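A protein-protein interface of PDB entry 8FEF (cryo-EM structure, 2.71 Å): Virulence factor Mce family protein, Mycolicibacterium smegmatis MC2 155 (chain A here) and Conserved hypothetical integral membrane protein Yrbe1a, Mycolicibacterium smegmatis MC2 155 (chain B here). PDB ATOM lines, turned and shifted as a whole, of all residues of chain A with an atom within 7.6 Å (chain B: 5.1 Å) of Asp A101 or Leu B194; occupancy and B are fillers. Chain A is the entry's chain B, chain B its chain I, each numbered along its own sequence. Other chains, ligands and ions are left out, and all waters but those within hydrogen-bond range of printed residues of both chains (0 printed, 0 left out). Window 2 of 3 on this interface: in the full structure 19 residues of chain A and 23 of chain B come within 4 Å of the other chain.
Among the printed residues, pairs that only touch across the chains: Phe A28 with Leu B192 (3.7 Å), Phe A28 with Thr B196 (3.5 Å), Asp A101 with Leu B194 (3.7 Å), Ile A103 with Leu B194 (3.9 Å) and Asn A105 with Leu B194 (3.5 Å).
The side-chain amide nitrogen of Gln A30 lies within hydrogen-bond range of the side-chain hydroxyl of Thr B193, at 3.4 Å.
Leu B194 touches three residues of chain A. Of the printed residues of chain A, Thr B193 touches Gln A30 (3.4 Å). Of the printed residues of chain B, Gln A30 touches Thr B193. Of the printed residues of chain A, Leu B192 touches Phe A28. Printed residues of chain B within 4 Å of Ile A103: Leu B194 (3.9 Å). The nearest residue of chain A that does not touch Leu B194 is Gln A100 (5.0 Å). The nearest printed residue of chain B that does not touch Phe A28 is Thr B193 (4.1 Å).
The side-chain carboxylate (OD1) of Asp A101 lies within hydrogen-bond range of the backbone NH (N) of Gly A104, 3.5 Å away. The backbone NH (N) of Gln A100 is in hydrogen-bond range of the backbone carbonyl oxygen (O) of Asn A105 (2.7 Å). OD1 of Asp A101 sits close to N of Ile A103 (3.5 Å). The side-chain amide nitrogen (ND2) of Asn A105 is in hydrogen-bond range of the side-chain carboxylate (OD2) of Asp A101.
Of the 9 printed residues of chain B, 4 touch a printed residue of chain A. Hydrophobic or aromatic side chains of chain B within 4 Å of the printed part of chain A: Leu B194. Printed residues of chain A that touch a printed residue of chain B: Phe A28, Gln A30, Asp A101, Ile A103 and Asn A105. Among the printed residues, no Asp or Glu carboxylate lies within 4 Å of a Lys or Arg side-chain nitrogen of the other chain.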
ATOM      1  N   PHE A  28      -5.320  -8.759  31.497  1.00  0.00           N
ATOM      2  CA  PHE A  28      -5.899  -7.745  30.626  1.00  0.00           C
ATOM      3  C   PHE A  28      -5.400  -6.337  30.917  1.00  0.00           C
ATOM      4  O   PHE A  28      -5.756  -5.410  30.185  1.00  0.00           O
ATOM      5  CB  PHE A  28      -7.425  -7.790  30.703  1.00  0.00           C
ATOM      6  CG  PHE A  28      -8.011  -9.025  30.095  1.00  0.00           C
ATOM      7  CD1 PHE A  28      -8.090  -9.156  28.720  1.00  0.00           C
ATOM      8  CD2 PHE A  28      -8.463 -10.061  30.889  1.00  0.00           C
ATOM      9  CE1 PHE A  28      -8.617 -10.289  28.150  1.00  0.00           C
ATOM     10  CE2 PHE A  28      -8.992 -11.198  30.322  1.00  0.00           C
ATOM     11  CZ  PHE A  28      -9.068 -11.311  28.948  1.00  0.00           C
ATOM     12  N   GLN A  30      -1.945  -5.812  31.374  1.00  0.00           N
ATOM     13  CA  GLN A  30      -0.549  -5.840  30.940  1.00  0.00           C
ATOM     14  C   GLN A  30       0.387  -5.393  32.065  1.00  0.00           C
ATOM     15  O   GLN A  30       1.101  -4.396  31.964  1.00  0.00           O
ATOM     16  CB  GLN A  30      -0.356  -4.991  29.678  1.00  0.00           C
ATOM     17  CG  GLN A  30      -1.222  -5.405  28.494  1.00  0.00           C
ATOM     18  CD  GLN A  30      -0.676  -6.603  27.740  1.00  0.00           C
ATOM     19  OE1 GLN A  30       0.259  -7.265  28.187  1.00  0.00           O
ATOM     20  NE2 GLN A  30      -1.259  -6.884  26.584  1.00  0.00           N
ATOM     21  N   ARG A  98       7.015   1.484  15.296  1.00  0.00           N
ATOM     22  CA  ARG A  98       6.587   0.510  14.308  1.00  0.00           C
ATOM     23  C   ARG A  98       5.120   0.153  14.499  1.00  0.00           C
ATOM     24  O   ARG A  98       4.593   0.181  15.616  1.00  0.00           O
ATOM     25  CB  ARG A  98       7.436  -0.763  14.391  1.00  0.00           C
ATOM     26  CG  ARG A  98       8.903  -0.577  14.039  1.00  0.00           C
ATOM     27  CD  ARG A  98       9.107  -0.447  12.540  1.00  0.00           C
ATOM     28  NE  ARG A  98       9.087   0.940  12.091  1.00  0.00           N
ATOM     29  CZ  ARG A  98      10.168   1.637  11.772  1.00  0.00           C
ATOM     30  NH1 ARG A  98      11.375   1.100  11.823  1.00  0.00           N
ATOM     31  NH2 ARG A  98      10.034   2.902  11.386  1.00  0.00           N
ATOM     32  N   TYR A  99       4.468  -0.172  13.382  1.00  0.00           N
ATOM     33  CA  TYR A  99       3.097  -0.664  13.412  1.00  0.00           C
ATOM     34  C   TYR A  99       3.019  -1.983  14.165  1.00  0.00           C
ATOM     35  O   TYR A  99       3.829  -2.886  13.944  1.00  0.00           O
ATOM     36  CB  TYR A  99       2.569  -0.872  11.991  1.00  0.00           C
ATOM     37  CG  TYR A  99       2.058   0.356  11.276  1.00  0.00           C
ATOM     38  CD1 TYR A  99       2.484   1.627  11.627  1.00  0.00           C
ATOM     39  CD2 TYR A  99       1.139   0.237  10.243  1.00  0.00           C
ATOM     40  CE1 TYR A  99       2.011   2.743  10.964  1.00  0.00           C
ATOM     41  CE2 TYR A  99       0.662   1.343   9.580  1.00  0.00           C
ATOM     42  CZ  TYR A  99       1.099   2.593   9.944  1.00  0.00           C
ATOM     43  OH  TYR A  99       0.622   3.698   9.281  1.00  0.00           O
ATOM     44  N   GLN A 100       2.037  -2.095  15.053  1.00  0.00           N
ATOM     45  CA  GLN A 100       1.690  -3.395  15.606  1.00  0.00           C
ATOM     46  C   GLN A 100       0.689  -4.126  14.725  1.00  0.00           C
ATOM     47  O   GLN A 100       0.761  -5.353  14.597  1.00  0.00           O
ATOM     48  CB  GLN A 100       1.130  -3.242  17.023  1.00  0.00           C
ATOM     49  CG  GLN A 100       0.695  -4.547  17.667  1.00  0.00           C
ATOM     50  CD  GLN A 100      -0.063  -4.338  18.961  1.00  0.00           C
ATOM     51  OE1 GLN A 100       0.115  -3.329  19.642  1.00  0.00           O
ATOM     52  NE2 GLN A 100      -0.919  -5.291  19.304  1.00  0.00           N
ATOM     53  N   ASP A 101      -0.217  -3.389  14.092  1.00  0.00           N
ATOM     54  CA  ASP A 101      -1.216  -3.956  13.197  1.00  0.00           C
ATOM     55  C   ASP A 101      -1.691  -2.854  12.255  1.00  0.00           C
ATOM     56  O   ASP A 101      -1.133  -1.752  12.230  1.00  0.00           O
ATOM     57  CB  ASP A 101      -2.367  -4.574  13.993  1.00  0.00           C
ATOM     58  CG  ASP A 101      -2.905  -3.646  15.068  1.00  0.00           C
ATOM     59  OD1 ASP A 101      -2.682  -2.422  14.979  1.00  0.00           O
ATOM     60  OD2 ASP A 101      -3.549  -4.141  16.014  1.00  0.00           O
ATOM     61  N   LEU A 102      -2.731  -3.151  11.482  1.00  0.00           N
ATOM     62  CA  LEU A 102      -3.286  -2.206  10.525  1.00  0.00           C
ATOM     63  C   LEU A 102      -4.487  -1.441  11.066  1.00  0.00           C
ATOM     64  O   LEU A 102      -5.154  -0.740  10.299  1.00  0.00           O
ATOM     65  CB  LEU A 102      -3.666  -2.930   9.232  1.00  0.00           C
ATOM     66  CG  LEU A 102      -2.513  -3.531   8.426  1.00  0.00           C
ATOM     67  CD1 LEU A 102      -3.034  -4.270   7.208  1.00  0.00           C
ATOM     68  CD2 LEU A 102      -1.528  -2.451   8.015  1.00  0.00           C
ATOM     69  N   ILE A 103      -4.786  -1.558  12.360  1.00  0.00           N
ATOM     70  CA  ILE A 103      -5.919  -0.857  12.953  1.00  0.00           C
ATOM     71  C   ILE A 103      -5.477   0.260  13.891  1.00  0.00           C
ATOM     72  O   ILE A 103      -6.317   0.866  14.563  1.00  0.00           O
ATOM     73  CB  ILE A 103      -6.873  -1.827  13.668  1.00  0.00           C
ATOM     74  CG1 ILE A 103      -6.148  -2.573  14.786  1.00  0.00           C
ATOM     75  CG2 ILE A 103      -7.477  -2.806  12.676  1.00  0.00           C
ATOM     76  CD1 ILE A 103      -7.023  -3.551  15.534  1.00  0.00           C
ATOM     77  N   GLY A 104      -4.180   0.554  13.956  1.00  0.00           N
ATOM     78  CA  GLY A 104      -3.724   1.732  14.668  1.00  0.00           C
ATOM     79  C   GLY A 104      -2.864   1.517  15.898  1.00  0.00           C
ATOM     80  O   GLY A 104      -2.565   2.479  16.610  1.00  0.00           O
ATOM     81  N   ASN A 105      -2.457   0.281  16.171  1.00  0.00           N
ATOM     82  CA  ASN A 105      -1.614  -0.001  17.324  1.00  0.00           C
ATOM     83  C   ASN A 105      -0.146   0.139  16.949  1.00  0.00           C
ATOM     84  O   ASN A 105       0.264  -0.233  15.846  1.00  0.00           O
ATOM     85  CB  ASN A 105      -1.889  -1.401  17.873  1.00  0.00           C
ATOM     86  CG  ASN A 105      -3.324  -1.581  18.317  1.00  0.00           C
ATOM     87  OD1 ASN A 105      -3.981  -0.627  18.731  1.00  0.00           O
ATOM     88  ND2 ASN A 105      -3.820  -2.807  18.236  1.00  0.00           N
ATOM     89  N   ARG A 106       0.645   0.673  17.875  1.00  0.00           N
ATOM     90  CA  ARG A 106       2.048   0.981  17.643  1.00  0.00           C
ATOM     91  C   ARG A 106       2.899   0.367  18.744  1.00  0.00           C
ATOM     92  O   ARG A 106       2.392  -0.109  19.761  1.00  0.00           O
ATOM     93  CB  ARG A 106       2.289   2.496  17.590  1.00  0.00           C
ATOM     94  CG  ARG A 106       1.388   3.253  16.637  1.00  0.00           C
ATOM     95  CD  ARG A 106       1.859   3.127  15.205  1.00  0.00           C
ATOM     96  NE  ARG A 106       0.989   3.856  14.292  1.00  0.00           N
ATOM     97  CZ  ARG A 106      -0.010   3.311  13.614  1.00  0.00           C
ATOM     98  NH1 ARG A 106      -0.281   2.020  13.704  1.00  0.00           N
ATOM     99  NH2 ARG A 106      -0.754   4.079  12.824  1.00  0.00           N
ATOM    100  N   TYR A 107       4.212   0.377  18.524  1.00  0.00           N
ATOM    101  CA  TYR A 107       5.157   0.029  19.577  1.00  0.00           C
ATOM    102  C   TYR A 107       6.491   0.698  19.285  1.00  0.00           C
ATOM    103  O   TYR A 107       6.735   1.184  18.178  1.00  0.00           O
ATOM    104  CB  TYR A 107       5.321  -1.492  19.728  1.00  0.00           C
ATOM    105  CG  TYR A 107       5.985  -2.206  18.568  1.00  0.00           C
ATOM    106  CD1 TYR A 107       7.365  -2.340  18.504  1.00  0.00           C
ATOM    107  CD2 TYR A 107       5.227  -2.769  17.551  1.00  0.00           C
ATOM    108  CE1 TYR A 107       7.971  -2.998  17.453  1.00  0.00           C
ATOM    109  CE2 TYR A 107       5.826  -3.429  16.498  1.00  0.00           C
ATOM    110  CZ  TYR A 107       7.196  -3.540  16.454  1.00  0.00           C
ATOM    111  OH  TYR A 107       7.796  -4.196  15.405  1.00  0.00           O
ATOM    112  N   VAL B  89      -8.623 -13.683  14.673  1.00  0.00           N
ATOM    113  CA  VAL B  89      -9.028 -12.627  15.593  1.00  0.00           C
ATOM    114  C   VAL B  89     -10.150 -13.083  16.517  1.00  0.00           C
ATOM    115  O   VAL B  89     -10.664 -12.282  17.307  1.00  0.00           O
ATOM    116  CB  VAL B  89      -9.431 -11.360  14.828  1.00  0.00           C
ATOM    117  CG1 VAL B  89      -8.228 -10.779  14.109  1.00  0.00           C
ATOM    118  CG2 VAL B  89     -10.536 -11.679  13.838  1.00  0.00           C
ATOM    119  N   ALA B  92     -10.130 -12.250  20.218  1.00  0.00           N
ATOM    120  CA  ALA B  92     -10.585 -10.900  20.541  1.00  0.00           C
ATOM    121  C   ALA B  92     -12.033 -10.920  21.000  1.00  0.00           C
ATOM    122  O   ALA B  92     -12.343 -10.569  22.145  1.00  0.00           O
ATOM    123  CB  ALA B  92     -10.433  -9.976  19.333  1.00  0.00           C
ATOM    124  N   THR B 191      -4.571 -12.426  20.871  1.00  0.00           N
ATOM    125  CA  THR B 191      -5.571 -11.462  20.444  1.00  0.00           C
ATOM    126  C   THR B 191      -6.573 -11.146  21.558  1.00  0.00           C
ATOM    127  O   THR B 191      -7.441 -10.284  21.382  1.00  0.00           O
ATOM    128  CB  THR B 191      -6.244 -12.013  19.168  1.00  0.00           C
ATOM    129  OG1 THR B 191      -5.236 -12.183  18.167  1.00  0.00           O
ATOM    130  CG2 THR B 191      -7.208 -11.039  18.549  1.00  0.00           C
ATOM    131  N   LEU B 192      -6.424 -11.768  22.733  1.00  0.00           N
ATOM    132  CA  LEU B 192      -7.347 -11.523  23.841  1.00  0.00           C
ATOM    133  C   LEU B 192      -7.335 -10.062  24.272  1.00  0.00           C
ATOM    134  O   LEU B 192      -8.389  -9.479  24.549  1.00  0.00           O
ATOM    135  CB  LEU B 192      -7.005 -12.417  25.033  1.00  0.00           C
ATOM    136  CG  LEU B 192      -7.276 -13.917  24.951  1.00  0.00           C
ATOM    137  CD1 LEU B 192      -6.796 -14.608  26.211  1.00  0.00           C
ATOM    138  CD2 LEU B 192      -8.754 -14.176  24.733  1.00  0.00           C
ATOM    139  N   THR B 193      -6.157  -9.451  24.326  1.00  0.00           N
ATOM    140  CA  THR B 193      -6.009  -8.076  24.779  1.00  0.00           C
ATOM    141  C   THR B 193      -6.191  -7.056  23.665  1.00  0.00           C
ATOM    142  O   THR B 193      -5.992  -5.861  23.905  1.00  0.00           O
ATOM    143  CB  THR B 193      -4.635  -7.884  25.426  1.00  0.00           C
ATOM    144  OG1 THR B 193      -3.614  -8.277  24.500  1.00  0.00           O
ATOM    145  CG2 THR B 193      -4.517  -8.728  26.684  1.00  0.00           C
ATOM    146  N   LEU B 194      -6.550  -7.496  22.456  1.00  0.00           N
ATOM    147  CA  LEU B 194      -6.709  -6.567  21.341  1.00  0.00           C
ATOM    148  C   LEU B 194      -7.852  -5.588  21.586  1.00  0.00           C
ATOM    149  O   LEU B 194      -7.727  -4.394  21.292  1.00  0.00           O
ATOM    150  CB  LEU B 194      -6.938  -7.342  20.044  1.00  0.00           C
ATOM    151  CG  LEU B 194      -7.068  -6.511  18.766  1.00  0.00           C
ATOM    152  CD1 LEU B 194      -5.795  -5.730  18.502  1.00  0.00           C
ATOM    153  CD2 LEU B 194      -7.413  -7.395  17.583  1.00  0.00           C
ATOM    154  N   LEU B 195      -8.971  -6.071  22.122  1.00  0.00           N
ATOM    155  CA  LEU B 195     -10.134  -5.231  22.368  1.00  0.00           C
ATOM    156  C   LEU B 195     -10.514  -5.130  23.838  1.00  0.00           C
ATOM    157  O   LEU B 195     -11.481  -4.432  24.161  1.00  0.00           O
ATOM    158  CB  LEU B 195     -11.340  -5.743  21.571  1.00  0.00           C
ATOM    159  CG  LEU B 195     -11.217  -5.753  20.047  1.00  0.00           C
ATOM    160  CD1 LEU B 195     -12.490  -6.286  19.416  1.00  0.00           C
ATOM    161  CD2 LEU B 195     -10.904  -4.362  19.528  1.00  0.00           C
ATOM    162  N   THR B 196      -9.793  -5.797  24.735  1.00  0.00           N
ATOM    163  CA  THR B 196     -10.115  -5.803  26.155  1.00  0.00           C
ATOM    164  C   THR B 196      -8.920  -5.295  26.947  1.00  0.00           C
ATOM    165  O   THR B 196      -7.792  -5.752  26.741  1.00  0.00           O
ATOM    166  CB  THR B 196     -10.501  -7.211  26.619  1.00  0.00           C
ATOM    167  OG1 THR B 196     -11.580  -7.700  25.816  1.00  0.00           O
ATOM    168  CG2 THR B 196     -10.940  -7.196  28.069  1.00  0.00           C
ATOM    169  N   THR B 264     -11.774   0.482  24.864  1.00  0.00           N
ATOM    170  CA  THR B 264     -10.359   0.212  24.639  1.00  0.00           C
ATOM    171  C   THR B 264      -9.939   0.562  23.216  1.00  0.00           C
ATOM    172  O   THR B 264      -8.856   1.119  23.005  1.00  0.00           O
ATOM    173  CB  THR B 264     -10.048  -1.260  24.937  1.00  0.00           C
ATOM    174  OG1 THR B 264     -10.193  -1.503  26.340  1.00  0.00           O
ATOM    175  CG2 THR B 264      -8.629  -1.619  24.519  1.00  0.00           C
